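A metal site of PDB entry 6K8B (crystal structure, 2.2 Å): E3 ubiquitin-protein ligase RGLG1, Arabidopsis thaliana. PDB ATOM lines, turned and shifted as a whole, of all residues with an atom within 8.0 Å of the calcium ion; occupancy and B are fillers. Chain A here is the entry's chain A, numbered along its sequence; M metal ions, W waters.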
ATOM      1  N   SER A  37      17.550  22.981 -14.281  1.00  0.00           N
ATOM      2  CA  SER A  37      16.449  23.931 -14.181  1.00  0.00           C
ATOM      3  C   SER A  37      16.148  24.557 -15.536  1.00  0.00           C
ATOM      4  O   SER A  37      17.003  24.541 -16.440  1.00  0.00           O
ATOM      5  CB  SER A  37      16.758  25.008 -13.142  1.00  0.00           C
ATOM      6  OG  SER A  37      17.717  25.932 -13.628  1.00  0.00           O
ATOM      7  N   ASN A  38      14.930  25.082 -15.692  1.00  0.00           N
ATOM      8  CA  ASN A  38      14.507  25.742 -16.920  1.00  0.00           C
ATOM      9  C   ASN A  38      13.674  26.984 -16.619  1.00  0.00           C
ATOM     10  O   ASN A  38      12.999  27.051 -15.597  1.00  0.00           O
ATOM     11  CB  ASN A  38      13.706  24.780 -17.824  1.00  0.00           C
ATOM     12  CG  ASN A  38      14.603  23.842 -18.609  1.00  0.00           C
ATOM     13  OD1 ASN A  38      15.194  24.223 -19.617  1.00  0.00           O
ATOM     14  ND2 ASN A  38      14.712  22.604 -18.138  1.00  0.00           N
ATOM     15  N   LEU A  39      13.747  27.972 -17.501  1.00  0.00           N
ATOM     16  CA  LEU A  39      13.016  29.217 -17.314  1.00  0.00           C
ATOM     17  C   LEU A  39      11.769  29.305 -18.196  1.00  0.00           C
ATOM     18  O   LEU A  39      11.698  28.713 -19.276  1.00  0.00           O
ATOM     19  CB  LEU A  39      13.914  30.418 -17.606  1.00  0.00           C
ATOM     20  CG  LEU A  39      15.148  30.567 -16.712  1.00  0.00           C
ATOM     21  CD1 LEU A  39      15.975  31.751 -17.161  1.00  0.00           C
ATOM     22  CD2 LEU A  39      14.748  30.695 -15.251  1.00  0.00           C
ATOM     23  N   ILE A  40      10.787  30.043 -17.687  1.00  0.00           N
ATOM     24  CA  ILE A  40       9.586  30.411 -18.417  1.00  0.00           C
ATOM     25  C   ILE A  40       9.435  31.933 -18.242  1.00  0.00           C
ATOM     26  O   ILE A  40       9.599  32.429 -17.123  1.00  0.00           O
ATOM     27  CB  ILE A  40       8.345  29.678 -17.891  1.00  0.00           C
ATOM     28  CG1 ILE A  40       8.583  28.166 -17.830  1.00  0.00           C
ATOM     29  CG2 ILE A  40       7.083  30.018 -18.726  1.00  0.00           C
ATOM     30  CD1 ILE A  40       7.434  27.397 -17.193  1.00  0.00           C
ATOM     31  N   ALA A  84      20.549  33.532 -17.129  1.00  0.00           N
ATOM     32  CA  ALA A  84      20.590  32.666 -18.304  1.00  0.00           C
ATOM     33  C   ALA A  84      21.076  31.248 -18.002  1.00  0.00           C
ATOM     34  O   ALA A  84      20.636  30.275 -18.651  1.00  0.00           O
ATOM     35  CB  ALA A  84      21.458  33.288 -19.386  1.00  0.00           C
ATOM     36  N   PHE A  86      20.405  29.504 -15.562  1.00  0.00           N
ATOM     37  CA  PHE A  86      19.344  28.725 -14.945  1.00  0.00           C
ATOM     38  C   PHE A  86      18.367  28.181 -15.970  1.00  0.00           C
ATOM     39  O   PHE A  86      17.403  27.523 -15.605  1.00  0.00           O
ATOM     40  CB  PHE A  86      18.605  29.558 -13.898  1.00  0.00           C
ATOM     41  CG  PHE A  86      19.402  29.779 -12.653  1.00  0.00           C
ATOM     42  CD1 PHE A  86      20.311  30.829 -12.574  1.00  0.00           C
ATOM     43  CD2 PHE A  86      19.287  28.894 -11.595  1.00  0.00           C
ATOM     44  CE1 PHE A  86      21.077  31.017 -11.441  1.00  0.00           C
ATOM     45  CE2 PHE A  86      20.066  29.066 -10.454  1.00  0.00           C
ATOM     46  CZ  PHE A  86      20.962  30.133 -10.382  1.00  0.00           C
ATOM     47  N   ASP A  87      18.609  28.449 -17.243  1.00  0.00           N
ATOM     48  CA  ASP A  87      17.922  27.671 -18.259  1.00  0.00           C
ATOM     49  C   ASP A  87      18.927  26.769 -18.981  1.00  0.00           C
ATOM     50  O   ASP A  87      19.827  27.248 -19.668  1.00  0.00           O
ATOM     51  CB  ASP A  87      17.215  28.564 -19.262  1.00  0.00           C
ATOM     52  CG  ASP A  87      16.308  27.772 -20.164  1.00  0.00           C
ATOM     53  OD1 ASP A  87      16.806  27.263 -21.188  1.00  0.00           O
ATOM     54  OD2 ASP A  87      15.111  27.621 -19.834  1.00  0.00           O
ATOM     55  N   GLU A  88      18.779  25.459 -18.812  1.00  0.00           N
ATOM     56  CA  GLU A  88      19.861  24.539 -19.143  1.00  0.00           C
ATOM     57  C   GLU A  88      20.147  24.409 -20.635  1.00  0.00           C
ATOM     58  O   GLU A  88      21.285  24.133 -21.014  1.00  0.00           O
ATOM     59  CB  GLU A  88      19.579  23.161 -18.546  1.00  0.00           C
ATOM     60  CG  GLU A  88      18.413  22.448 -19.178  1.00  0.00           C
ATOM     61  CD  GLU A  88      18.096  21.133 -18.495  1.00  0.00           C
ATOM     62  OE1 GLU A  88      18.839  20.720 -17.558  1.00  0.00           O
ATOM     63  OE2 GLU A  88      17.096  20.499 -18.901  1.00  0.00           O
ATOM     64  N   ASP A  89      19.146  24.608 -21.486  1.00  0.00           N
ATOM     65  CA  ASP A  89      19.354  24.483 -22.932  1.00  0.00           C
ATOM     66  C   ASP A  89      19.238  25.820 -23.691  1.00  0.00           C
ATOM     67  O   ASP A  89      19.262  25.838 -24.926  1.00  0.00           O
ATOM     68  CB  ASP A  89      18.354  23.475 -23.513  1.00  0.00           C
ATOM     69  CG  ASP A  89      16.907  23.846 -23.217  1.00  0.00           C
ATOM     70  OD1 ASP A  89      16.641  24.951 -22.696  1.00  0.00           O
ATOM     71  OD2 ASP A  89      16.017  23.025 -23.520  1.00  0.00           O
ATOM     72  N   ASN A  90      19.123  26.927 -22.955  1.00  0.00           N
ATOM     73  CA  ASN A  90      19.007  28.265 -23.531  1.00  0.00           C
ATOM     74  C   ASN A  90      17.813  28.410 -24.495  1.00  0.00           C
ATOM     75  O   ASN A  90      17.816  29.264 -25.389  1.00  0.00           O
ATOM     76  CB  ASN A  90      20.324  28.644 -24.233  1.00  0.00           C
ATOM     77  CG  ASN A  90      20.523  30.150 -24.354  1.00  0.00           C
ATOM     78  OD1 ASN A  90      20.332  30.909 -23.396  1.00  0.00           O
ATOM     79  ND2 ASN A  90      20.924  30.584 -25.540  1.00  0.00           N
ATOM     80  N   LEU A  91      16.801  27.572 -24.315  1.00  0.00           N
ATOM     81  CA  LEU A  91      15.545  27.663 -25.063  1.00  0.00           C
ATOM     82  C   LEU A  91      14.438  28.107 -24.116  1.00  0.00           C
ATOM     83  O   LEU A  91      14.114  27.404 -23.173  1.00  0.00           O
ATOM     84  CB  LEU A  91      15.188  26.308 -25.700  1.00  0.00           C
ATOM     85  CG  LEU A  91      16.091  25.889 -26.868  1.00  0.00           C
ATOM     86  CD1 LEU A  91      15.979  24.393 -27.125  1.00  0.00           C
ATOM     87  CD2 LEU A  91      15.735  26.701 -28.110  1.00  0.00           C
ATOM     88  N   ILE A  92      13.879  29.284 -24.364  1.00  0.00           N
ATOM     89  CA  ILE A  92      12.991  29.873 -23.378  1.00  0.00           C
ATOM     90  C   ILE A  92      11.603  30.096 -23.955  1.00  0.00           C
ATOM     91  O   ILE A  92      11.432  30.891 -24.870  1.00  0.00           O
ATOM     92  CB  ILE A  92      13.552  31.229 -22.842  1.00  0.00           C
ATOM     93  CG1 ILE A  92      14.872  31.019 -22.095  1.00  0.00           C
ATOM     94  CG2 ILE A  92      12.559  31.889 -21.902  1.00  0.00           C
ATOM     95  CD1 ILE A  92      16.086  31.110 -22.972  1.00  0.00           C
ATOM     96  N   PRO A  93      10.603  29.364 -23.428  1.00  0.00           N
ATOM     97  CA  PRO A  93       9.205  29.598 -23.791  1.00  0.00           C
ATOM     98  C   PRO A  93       8.742  30.947 -23.236  1.00  0.00           C
ATOM     99  O   PRO A  93       8.902  31.202 -22.036  1.00  0.00           O
ATOM    100  CB  PRO A  93       8.448  28.437 -23.126  1.00  0.00           C
ATOM    101  CG  PRO A  93       9.371  27.977 -22.017  1.00  0.00           C
ATOM    102  CD  PRO A  93      10.763  28.257 -22.484  1.00  0.00           C
ATOM    103  N   PHE A 116      10.245  28.037 -29.245  1.00  0.00           N
ATOM    104  CA  PHE A 116      10.847  28.745 -28.108  1.00  0.00           C
ATOM    105  C   PHE A 116      11.895  29.755 -28.586  1.00  0.00           C
ATOM    106  O   PHE A 116      12.519  29.570 -29.619  1.00  0.00           O
ATOM    107  CB  PHE A 116      11.509  27.765 -27.123  1.00  0.00           C
ATOM    108  CG  PHE A 116      10.554  26.776 -26.486  1.00  0.00           C
ATOM    109  CD1 PHE A 116       9.184  26.898 -26.628  1.00  0.00           C
ATOM    110  CD2 PHE A 116      11.051  25.728 -25.714  1.00  0.00           C
ATOM    111  CE1 PHE A 116       8.319  25.980 -26.041  1.00  0.00           C
ATOM    112  CE2 PHE A 116      10.195  24.812 -25.122  1.00  0.00           C
ATOM    113  CZ  PHE A 116       8.826  24.932 -25.287  1.00  0.00           C
ATOM    114  N   CYS A 117      12.077  30.819 -27.818  1.00  0.00           N
ATOM    115  CA  CYS A 117      13.168  31.750 -28.101  1.00  0.00           C
ATOM    116  C   CYS A 117      14.512  31.108 -27.806  1.00  0.00           C
ATOM    117  O   CYS A 117      14.709  30.481 -26.766  1.00  0.00           O
ATOM    118  CB  CYS A 117      13.014  33.041 -27.300  1.00  0.00           C
ATOM    119  SG  CYS A 117      11.584  34.048 -27.758  1.00  0.00           S
ATOM    120  N   HIS A 161      10.911  24.240 -12.779  1.00  0.00           N
ATOM    121  CA  HIS A 161      10.906  25.454 -13.594  1.00  0.00           C
ATOM    122  C   HIS A 161      10.836  26.713 -12.734  1.00  0.00           C
ATOM    123  O   HIS A 161      10.266  26.701 -11.642  1.00  0.00           O
ATOM    124  CB  HIS A 161       9.714  25.462 -14.586  1.00  0.00           C
ATOM    125  CG  HIS A 161       9.919  24.594 -15.794  1.00  0.00           C
ATOM    126  ND1 HIS A 161       9.880  23.215 -15.749  1.00  0.00           N
ATOM    127  CD2 HIS A 161      10.171  24.914 -17.093  1.00  0.00           C
ATOM    128  CE1 HIS A 161      10.082  22.721 -16.957  1.00  0.00           C
ATOM    129  NE2 HIS A 161      10.275  23.735 -17.792  1.00  0.00           N
HETATM  130 CA    CA M   1      14.688  25.960 -21.514  1.00  0.00          CA
HETATM  131  O   HOH W   1      13.498  23.986 -22.356  1.00  0.00           O
HETATM  132  O   HOH W   2      12.491  26.407 -20.483  1.00  0.00           O
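The calcium ion is bound by O of Leu 91, OD2 of Asp 87, water W1, water W2, OD1 of Asp 89, OD1 of Asp 87 and OD1 of Asn 38.
The calcium ion has seven donor atoms within binding distance.
Within 4 Å of the calcium ion: Asn 38, Asp 87, Asp 89 and Leu 91.
The nearest printed residue that does not touch the calcium ion is Ile 92 (4.5 Å).
N of Leu 39 lies close to OD2 of Asp 87, at 2.7 Å.
The side-chain carboxylate (OD1) of Asp 87 lies close to the backbone NH (N) of Asn 90.
The side-chain amide nitrogen (ND2) of Asn 38 lies within hydrogen-bond range of the side-chain carboxylate (OE2) of Glu 88.
The backbone carbonyl oxygen of Phe 86 sits at hydrogen-bond distance from the backbone NH of Asn 38, at 3.5 Å.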
